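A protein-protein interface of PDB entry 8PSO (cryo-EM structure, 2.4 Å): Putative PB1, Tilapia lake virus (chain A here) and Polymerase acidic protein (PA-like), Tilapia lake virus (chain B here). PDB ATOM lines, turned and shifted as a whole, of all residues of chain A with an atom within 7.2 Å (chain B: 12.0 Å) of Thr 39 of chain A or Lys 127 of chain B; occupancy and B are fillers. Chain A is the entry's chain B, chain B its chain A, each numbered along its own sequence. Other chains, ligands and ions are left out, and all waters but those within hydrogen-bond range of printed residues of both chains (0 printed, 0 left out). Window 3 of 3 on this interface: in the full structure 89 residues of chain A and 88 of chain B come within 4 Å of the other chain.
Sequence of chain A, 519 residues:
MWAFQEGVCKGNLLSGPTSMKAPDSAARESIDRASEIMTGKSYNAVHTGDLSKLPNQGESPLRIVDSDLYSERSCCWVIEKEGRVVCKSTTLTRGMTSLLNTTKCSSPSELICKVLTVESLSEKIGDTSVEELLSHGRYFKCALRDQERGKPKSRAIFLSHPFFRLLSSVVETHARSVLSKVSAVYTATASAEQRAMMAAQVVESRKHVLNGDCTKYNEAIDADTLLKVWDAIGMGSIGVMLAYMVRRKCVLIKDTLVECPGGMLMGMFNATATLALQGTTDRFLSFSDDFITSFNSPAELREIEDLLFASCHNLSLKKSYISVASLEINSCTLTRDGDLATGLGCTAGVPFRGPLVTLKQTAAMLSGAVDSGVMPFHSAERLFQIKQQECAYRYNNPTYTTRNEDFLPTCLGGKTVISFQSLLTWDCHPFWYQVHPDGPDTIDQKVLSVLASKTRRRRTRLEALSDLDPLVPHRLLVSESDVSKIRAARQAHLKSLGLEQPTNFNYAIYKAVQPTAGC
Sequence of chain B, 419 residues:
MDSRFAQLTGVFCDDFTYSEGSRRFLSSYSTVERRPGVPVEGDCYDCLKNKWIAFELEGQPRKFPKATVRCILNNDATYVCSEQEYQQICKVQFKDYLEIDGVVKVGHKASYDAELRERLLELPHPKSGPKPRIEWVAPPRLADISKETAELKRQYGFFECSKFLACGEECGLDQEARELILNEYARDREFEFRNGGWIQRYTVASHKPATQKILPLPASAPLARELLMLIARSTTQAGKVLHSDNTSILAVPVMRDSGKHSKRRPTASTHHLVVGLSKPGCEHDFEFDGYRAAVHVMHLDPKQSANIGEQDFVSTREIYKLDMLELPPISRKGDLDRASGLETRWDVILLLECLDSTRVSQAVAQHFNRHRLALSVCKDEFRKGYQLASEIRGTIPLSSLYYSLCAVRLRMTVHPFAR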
ATOM      1  N   ARG A  33      -9.928 -26.278   0.210  1.00  0.00           N
ATOM      2  CA  ARG A  33      -8.660 -26.070  -0.479  1.00  0.00           C
ATOM      3  C   ARG A  33      -8.375 -24.585  -0.663  1.00  0.00           C
ATOM      4  O   ARG A  33      -7.245 -24.127  -0.446  1.00  0.00           O
ATOM      5  CB  ARG A  33      -8.680 -26.778  -1.833  1.00  0.00           C
ATOM      6  CG  ARG A  33      -7.450 -27.620  -2.116  1.00  0.00           C
ATOM      7  CD  ARG A  33      -7.762 -28.761  -3.069  1.00  0.00           C
ATOM      8  NE  ARG A  33      -8.712 -28.358  -4.100  1.00  0.00           N
ATOM      9  CZ  ARG A  33      -9.711 -29.106  -4.551  1.00  0.00           C
ATOM     10  NH1 ARG A  33      -9.887 -30.350  -4.138  1.00  0.00           N
ATOM     11  NH2 ARG A  33     -10.543 -28.598  -5.454  1.00  0.00           N
ATOM     12  N   ALA A  34      -9.389 -23.816  -1.063  1.00  0.00           N
ATOM     13  CA  ALA A  34      -9.201 -22.376  -1.212  1.00  0.00           C
ATOM     14  C   ALA A  34      -8.839 -21.734   0.123  1.00  0.00           C
ATOM     15  O   ALA A  34      -7.957 -20.868   0.189  1.00  0.00           O
ATOM     16  CB  ALA A  34     -10.462 -21.737  -1.791  1.00  0.00           C
ATOM     17  N   SER A  35      -9.508 -22.151   1.200  1.00  0.00           N
ATOM     18  CA  SER A  35      -9.208 -21.601   2.518  1.00  0.00           C
ATOM     19  C   SER A  35      -7.780 -21.926   2.935  1.00  0.00           C
ATOM     20  O   SER A  35      -7.081 -21.077   3.498  1.00  0.00           O
ATOM     21  CB  SER A  35     -10.202 -22.142   3.546  1.00  0.00           C
ATOM     22  OG  SER A  35     -11.433 -21.448   3.476  1.00  0.00           O
ATOM     23  N   GLU A  36      -7.332 -23.155   2.673  1.00  0.00           N
ATOM     24  CA  GLU A  36      -5.958 -23.525   2.996  1.00  0.00           C
ATOM     25  C   GLU A  36      -4.967 -22.691   2.197  1.00  0.00           C
ATOM     26  O   GLU A  36      -3.938 -22.260   2.728  1.00  0.00           O
ATOM     27  CB  GLU A  36      -5.741 -25.014   2.732  1.00  0.00           C
ATOM     28  CG  GLU A  36      -4.541 -25.597   3.457  1.00  0.00           C
ATOM     29  CD  GLU A  36      -4.114 -26.938   2.895  1.00  0.00           C
ATOM     30  OE1 GLU A  36      -4.975 -27.834   2.771  1.00  0.00           O
ATOM     31  OE2 GLU A  36      -2.917 -27.097   2.577  1.00  0.00           O
ATOM     32  N   ILE A  37      -5.258 -22.456   0.916  1.00  0.00           N
ATOM     33  CA  ILE A  37      -4.378 -21.618   0.105  1.00  0.00           C
ATOM     34  C   ILE A  37      -4.326 -20.204   0.671  1.00  0.00           C
ATOM     35  O   ILE A  37      -3.269 -19.560   0.675  1.00  0.00           O
ATOM     36  CB  ILE A  37      -4.834 -21.627  -1.366  1.00  0.00           C
ATOM     37  CG1 ILE A  37      -4.595 -23.011  -1.977  1.00  0.00           C
ATOM     38  CG2 ILE A  37      -4.099 -20.543  -2.158  1.00  0.00           C
ATOM     39  CD1 ILE A  37      -4.996 -23.131  -3.434  1.00  0.00           C
ATOM     40  N   MET A  38      -5.461 -19.698   1.160  1.00  0.00           N
ATOM     41  CA  MET A  38      -5.471 -18.362   1.749  1.00  0.00           C
ATOM     42  C   MET A  38      -4.511 -18.260   2.927  1.00  0.00           C
ATOM     43  O   MET A  38      -3.951 -17.188   3.180  1.00  0.00           O
ATOM     44  CB  MET A  38      -6.884 -17.992   2.199  1.00  0.00           C
ATOM     45  CG  MET A  38      -7.800 -17.549   1.074  1.00  0.00           C
ATOM     46  SD  MET A  38      -7.456 -15.871   0.513  1.00  0.00           S
ATOM     47  CE  MET A  38      -8.101 -14.910   1.879  1.00  0.00           C
ATOM     48  N   THR A  39      -4.309 -19.358   3.659  1.00  0.00           N
ATOM     49  CA  THR A  39      -3.419 -19.329   4.812  1.00  0.00           C
ATOM     50  C   THR A  39      -1.954 -19.214   4.406  1.00  0.00           C
ATOM     51  O   THR A  39      -1.136 -18.753   5.208  1.00  0.00           O
ATOM     52  CB  THR A  39      -3.641 -20.581   5.671  1.00  0.00           C
ATOM     53  OG1 THR A  39      -4.796 -20.396   6.500  1.00  0.00           O
ATOM     54  CG2 THR A  39      -2.441 -20.861   6.559  1.00  0.00           C
ATOM     55  N   GLY A  40      -1.607 -19.604   3.183  1.00  0.00           N
ATOM     56  CA  GLY A  40      -0.239 -19.498   2.723  1.00  0.00           C
ATOM     57  C   GLY A  40       0.631 -20.700   3.005  1.00  0.00           C
ATOM     58  O   GLY A  40       1.859 -20.562   3.052  1.00  0.00           O
ATOM     59  N   LYS A  41       0.040 -21.879   3.199  1.00  0.00           N
ATOM     60  CA  LYS A  41       0.794 -23.090   3.486  1.00  0.00           C
ATOM     61  C   LYS A  41       0.768 -24.112   2.359  1.00  0.00           C
ATOM     62  O   LYS A  41       1.546 -25.071   2.405  1.00  0.00           O
ATOM     63  CB  LYS A  41       0.262 -23.760   4.766  1.00  0.00           C
ATOM     64  CG  LYS A  41       0.659 -23.105   6.098  1.00  0.00           C
ATOM     65  CD  LYS A  41       2.010 -22.404   6.069  1.00  0.00           C
ATOM     66  CE  LYS A  41       2.363 -21.841   7.435  1.00  0.00           C
ATOM     67  NZ  LYS A  41       3.680 -21.148   7.436  1.00  0.00           N
ATOM     68  N   SER A  42      -0.092 -23.942   1.354  1.00  0.00           N
ATOM     69  CA  SER A  42      -0.240 -24.923   0.285  1.00  0.00           C
ATOM     70  C   SER A  42       0.223 -24.387  -1.064  1.00  0.00           C
ATOM     71  O   SER A  42       1.085 -24.992  -1.707  1.00  0.00           O
ATOM     72  CB  SER A  42      -1.704 -25.378   0.199  1.00  0.00           C
ATOM     73  OG  SER A  42      -1.794 -26.719  -0.247  1.00  0.00           O
ATOM     74  N   TYR A  43      -0.328 -23.262  -1.512  1.00  0.00           N
ATOM     75  CA  TYR A  43      -0.001 -22.707  -2.816  1.00  0.00           C
ATOM     76  C   TYR A  43      -0.029 -21.189  -2.733  1.00  0.00           C
ATOM     77  O   TYR A  43      -0.648 -20.606  -1.840  1.00  0.00           O
ATOM     78  CB  TYR A  43      -0.968 -23.197  -3.902  1.00  0.00           C
ATOM     79  CG  TYR A  43      -0.838 -24.669  -4.212  1.00  0.00           C
ATOM     80  CD1 TYR A  43       0.195 -25.141  -5.010  1.00  0.00           C
ATOM     81  CD2 TYR A  43      -1.746 -25.588  -3.703  1.00  0.00           C
ATOM     82  CE1 TYR A  43       0.320 -26.486  -5.293  1.00  0.00           C
ATOM     83  CE2 TYR A  43      -1.628 -26.934  -3.982  1.00  0.00           C
ATOM     84  CZ  TYR A  43      -0.595 -27.378  -4.777  1.00  0.00           C
ATOM     85  OH  TYR A  43      -0.476 -28.719  -5.056  1.00  0.00           O
ATOM     86  N   ASN A  44       0.652 -20.555  -3.682  1.00  0.00           N
ATOM     87  CA  ASN A  44       0.754 -19.105  -3.699  1.00  0.00           C
ATOM     88  C   ASN A  44      -0.496 -18.492  -4.318  1.00  0.00           C
ATOM     89  O   ASN A  44      -0.931 -18.900  -5.399  1.00  0.00           O
ATOM     90  CB  ASN A  44       1.995 -18.670  -4.474  1.00  0.00           C
ATOM     91  CG  ASN A  44       2.251 -17.182  -4.375  1.00  0.00           C
ATOM     92  OD1 ASN A  44       2.178 -16.600  -3.293  1.00  0.00           O
ATOM     93  ND2 ASN A  44       2.546 -16.555  -5.506  1.00  0.00           N
ATOM     94  N   ALA A  45      -1.073 -17.510  -3.623  1.00  0.00           N
ATOM     95  CA  ALA A  45      -2.204 -16.748  -4.136  1.00  0.00           C
ATOM     96  C   ALA A  45      -1.939 -15.248  -4.117  1.00  0.00           C
ATOM     97  O   ALA A  45      -2.876 -14.463  -4.301  1.00  0.00           O
ATOM     98  CB  ALA A  45      -3.473 -17.062  -3.337  1.00  0.00           C
ATOM     99  N   VAL A  46      -0.695 -14.829  -3.900  1.00  0.00           N
ATOM    100  CA  VAL A  46      -0.321 -13.420  -3.885  1.00  0.00           C
ATOM    101  C   VAL A  46       0.384 -13.109  -5.197  1.00  0.00           C
ATOM    102  O   VAL A  46       1.427 -13.698  -5.505  1.00  0.00           O
ATOM    103  CB  VAL A  46       0.576 -13.090  -2.681  1.00  0.00           C
ATOM    104  CG1 VAL A  46       0.950 -11.614  -2.681  1.00  0.00           C
ATOM    105  CG2 VAL A  46      -0.118 -13.470  -1.380  1.00  0.00           C
ATOM    106  N   GLU B 122     -10.320  -3.641   4.465  1.00  0.00           N
ATOM    107  CA  GLU B 122     -10.589  -4.221   5.775  1.00  0.00           C
ATOM    108  C   GLU B 122     -10.814  -5.726   5.711  1.00  0.00           C
ATOM    109  O   GLU B 122     -10.680  -6.402   6.736  1.00  0.00           O
ATOM    110  CB  GLU B 122     -11.812  -3.549   6.408  1.00  0.00           C
ATOM    111  CG  GLU B 122     -11.691  -2.042   6.630  1.00  0.00           C
ATOM    112  CD  GLU B 122     -10.258  -1.559   6.755  1.00  0.00           C
ATOM    113  OE1 GLU B 122      -9.506  -2.121   7.579  1.00  0.00           O
ATOM    114  OE2 GLU B 122      -9.883  -0.617   6.027  1.00  0.00           O
ATOM    115  N   LEU B 123     -11.145  -6.265   4.543  1.00  0.00           N
ATOM    116  CA  LEU B 123     -11.400  -7.688   4.403  1.00  0.00           C
ATOM    117  C   LEU B 123     -10.089  -8.469   4.335  1.00  0.00           C
ATOM    118  O   LEU B 123      -9.039  -7.913   4.004  1.00  0.00           O
ATOM    119  CB  LEU B 123     -12.244  -7.944   3.158  1.00  0.00           C
ATOM    120  CG  LEU B 123     -13.740  -7.683   3.360  1.00  0.00           C
ATOM    121  CD1 LEU B 123     -14.413  -7.282   2.057  1.00  0.00           C
ATOM    122  CD2 LEU B 123     -14.418  -8.905   3.960  1.00  0.00           C
ATOM    123  N   PRO B 124     -10.123  -9.764   4.646  1.00  0.00           N
ATOM    124  CA  PRO B 124      -8.877 -10.537   4.719  1.00  0.00           C
ATOM    125  C   PRO B 124      -8.215 -10.694   3.358  1.00  0.00           C
ATOM    126  O   PRO B 124      -8.850 -10.610   2.305  1.00  0.00           O
ATOM    127  CB  PRO B 124      -9.315 -11.896   5.279  1.00  0.00           C
ATOM    128  CG  PRO B 124     -10.788 -11.950   5.153  1.00  0.00           C
ATOM    129  CD  PRO B 124     -11.320 -10.575   4.926  1.00  0.00           C
ATOM    130  N   HIS B 125      -6.906 -10.927   3.401  1.00  0.00           N
ATOM    131  CA  HIS B 125      -6.078 -11.091   2.218  1.00  0.00           C
ATOM    132  C   HIS B 125      -5.253 -12.364   2.332  1.00  0.00           C
ATOM    133  O   HIS B 125      -4.953 -12.816   3.441  1.00  0.00           O
ATOM    134  CB  HIS B 125      -5.139  -9.891   2.029  1.00  0.00           C
ATOM    135  CG  HIS B 125      -5.839  -8.569   2.037  1.00  0.00           C
ATOM    136  ND1 HIS B 125      -6.275  -7.951   0.885  1.00  0.00           N
ATOM    137  CD2 HIS B 125      -6.180  -7.747   3.057  1.00  0.00           C
ATOM    138  CE1 HIS B 125      -6.854  -6.805   1.196  1.00  0.00           C
ATOM    139  NE2 HIS B 125      -6.810  -6.658   2.507  1.00  0.00           N
ATOM    140  N   PRO B 126      -4.872 -12.962   1.204  1.00  0.00           N
ATOM    141  CA  PRO B 126      -4.081 -14.195   1.261  1.00  0.00           C
ATOM    142  C   PRO B 126      -2.666 -13.946   1.758  1.00  0.00           C
ATOM    143  O   PRO B 126      -2.097 -12.865   1.582  1.00  0.00           O
ATOM    144  CB  PRO B 126      -4.077 -14.682  -0.191  1.00  0.00           C
ATOM    145  CG  PRO B 126      -4.266 -13.451  -0.998  1.00  0.00           C
ATOM    146  CD  PRO B 126      -5.136 -12.540  -0.183  1.00  0.00           C
ATOM    147  N   LYS B 127      -2.099 -14.971   2.385  1.00  0.00           N
ATOM    148  CA  LYS B 127      -0.700 -14.962   2.778  1.00  0.00           C
ATOM    149  C   LYS B 127       0.152 -15.537   1.655  1.00  0.00           C
ATOM    150  O   LYS B 127      -0.298 -16.387   0.881  1.00  0.00           O
ATOM    151  CB  LYS B 127      -0.481 -15.770   4.059  1.00  0.00           C
ATOM    152  CG  LYS B 127      -1.489 -15.501   5.175  1.00  0.00           C
ATOM    153  CD  LYS B 127      -0.964 -14.510   6.205  1.00  0.00           C
ATOM    154  CE  LYS B 127      -1.313 -14.944   7.620  1.00  0.00           C
ATOM    155  NZ  LYS B 127      -2.768 -14.818   7.906  1.00  0.00           N
ATOM    156  N   SER B 128       1.393 -15.066   1.569  1.00  0.00           N
ATOM    157  CA  SER B 128       2.292 -15.537   0.525  1.00  0.00           C
ATOM    158  C   SER B 128       2.581 -17.022   0.709  1.00  0.00           C
ATOM    159  O   SER B 128       2.926 -17.470   1.806  1.00  0.00           O
ATOM    160  CB  SER B 128       3.593 -14.737   0.550  1.00  0.00           C
ATOM    161  OG  SER B 128       4.338 -14.937  -0.638  1.00  0.00           O
ATOM    162  N   GLY B 129       2.437 -17.784  -0.372  1.00  0.00           N
ATOM    163  CA  GLY B 129       2.684 -19.205  -0.338  1.00  0.00           C
ATOM    164  C   GLY B 129       4.152 -19.535  -0.522  1.00  0.00           C
ATOM    165  O   GLY B 129       4.934 -18.724  -1.027  1.00  0.00           O
ATOM    166  N   PRO B 130       4.555 -20.734  -0.112  1.00  0.00           N
ATOM    167  CA  PRO B 130       5.957 -21.130  -0.276  1.00  0.00           C
ATOM    168  C   PRO B 130       6.306 -21.384  -1.734  1.00  0.00           C
ATOM    169  O   PRO B 130       5.464 -21.780  -2.542  1.00  0.00           O
ATOM    170  CB  PRO B 130       6.061 -22.415   0.553  1.00  0.00           C
ATOM    171  CG  PRO B 130       4.683 -22.978   0.546  1.00  0.00           C
ATOM    172  CD  PRO B 130       3.741 -21.807   0.486  1.00  0.00           C
ATOM    173  N   LYS B 131       7.570 -21.150  -2.060  1.00  0.00           N
ATOM    174  CA  LYS B 131       8.066 -21.448  -3.399  1.00  0.00           C
ATOM    175  C   LYS B 131       8.439 -22.925  -3.489  1.00  0.00           C
ATOM    176  O   LYS B 131       9.225 -23.407  -2.667  1.00  0.00           O
ATOM    177  CB  LYS B 131       9.275 -20.583  -3.730  1.00  0.00           C
ATOM    178  CG  LYS B 131       9.633 -20.568  -5.206  1.00  0.00           C
ATOM    179  CD  LYS B 131       9.840 -19.154  -5.721  1.00  0.00           C
ATOM    180  CE  LYS B 131      10.647 -19.148  -7.007  1.00  0.00           C
ATOM    181  NZ  LYS B 131      12.093 -19.408  -6.766  1.00  0.00           N
ATOM    182  N   PRO B 132       7.907 -23.671  -4.455  1.00  0.00           N
ATOM    183  CA  PRO B 132       8.223 -25.099  -4.531  1.00  0.00           C
ATOM    184  C   PRO B 132       9.544 -25.362  -5.234  1.00  0.00           C
ATOM    185  O   PRO B 132       9.943 -24.653  -6.159  1.00  0.00           O
ATOM    186  CB  PRO B 132       7.050 -25.677  -5.330  1.00  0.00           C
ATOM    187  CG  PRO B 132       6.526 -24.536  -6.149  1.00  0.00           C
ATOM    188  CD  PRO B 132       7.047 -23.243  -5.573  1.00  0.00           C
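Of the 14 printed residues of chain A, 7 touch a printed residue of chain B. Hydrophobic or aromatic side chains of chain A that line the printed part of chain B: Met 38, Ala 45 and Val 46. Printed residues of chain B that touch a printed residue of chain A: His 125, Pro 126, Lys 127, Ser 128, Gly 129 and Pro 130. Among the printed residues, no Asp or Glu carboxylate lies within 4 Å of a Lys or Arg side-chain nitrogen of the other chain.
Thr 39 of chain A touches just one residue of chain B: Lys 127. Lys 127 of chain B touches four residues of chain A. No residue of chain B comes within 4 Å of Ser 35 of chain A. No residue of chain B comes within 4 Å of Glu 36 of chain A. Met 38 of chain A touches just these residues of chain B: His 125 (3.8 Å), Pro 126 (3.6 Å) and Lys 127 (3.0 Å). No residue of chain B comes within 4 Å of Lys 41 of chain A. Of chain B, only Ser 128 and Gly 129 come within 4 Å of Asn 44 of chain A. Printed residues of chain B within 4 Å of Val 46 of chain A: Pro 126 (3.6 Å), Lys 127 (3.7 Å) and Ser 128 (3.7 Å). Of the printed residues of chain B, Tyr 43 of chain A touches Gly 129. Of the printed residues of chain A, Ser 128 of chain B touches Gly 40 (3.5 Å), Asn 44 (3.8 Å) and Val 46 (3.7 Å). Of the printed residues of chain A, Pro 130 of chain B touches Gly 40 (3.4 Å). Printed residues of chain A within 4 Å of His 125 of chain B: Met 38. The nearest printed residue of chain B that does not touch Tyr 43 of chain A is Pro 130 of chain B (4.8 Å).
Among the printed residues, merely in contact across the chains: Thr 39 of chain A with Lys 127 of chain B (3.3 Å), Gly 40 of chain A with Pro 130 of chain B (3.4 Å), Gly 40 of chain A with Ser 128 of chain B (3.5 Å), Met 38 of chain A with Pro 126 of chain B (3.6 Å), Val 46 of chain A with Pro 126 of chain B (3.6 Å), Gly 40 of chain A with Lys 127 of chain B (3.6 Å), Val 46 of chain A with Ser 128 of chain B (3.7 Å), Val 46 of chain A with Lys 127 of chain B (3.7 Å), Ala 45 of chain A with Pro 126 of chain B (3.7 Å), Gly 40 of chain A with Gly 129 of chain B (3.7 Å), Asn 44 of chain A with Ser 128 of chain B (3.8 Å), Met 38 of chain A with His 125 of chain B (3.8 Å) and Tyr 43 of chain A with Gly 129 of chain B (3.9 Å).
NE2 of His 125 of chain B sits at hydrogen-bond distance from O of Leu 123 of chain B. ND2 of Asn 44 of chain A sits at hydrogen-bond distance from O of Val 46 of chain A.
The backbone NH (N) of Lys 127 of chain B lies within hydrogen-bond range of the backbone carbonyl oxygen (O) of Met 38 of chain A, at 3.0 Å. N of Gly 129 of chain B lies within hydrogen-bond range of OD1 of Asn 44 of chain A (3.2 Å).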
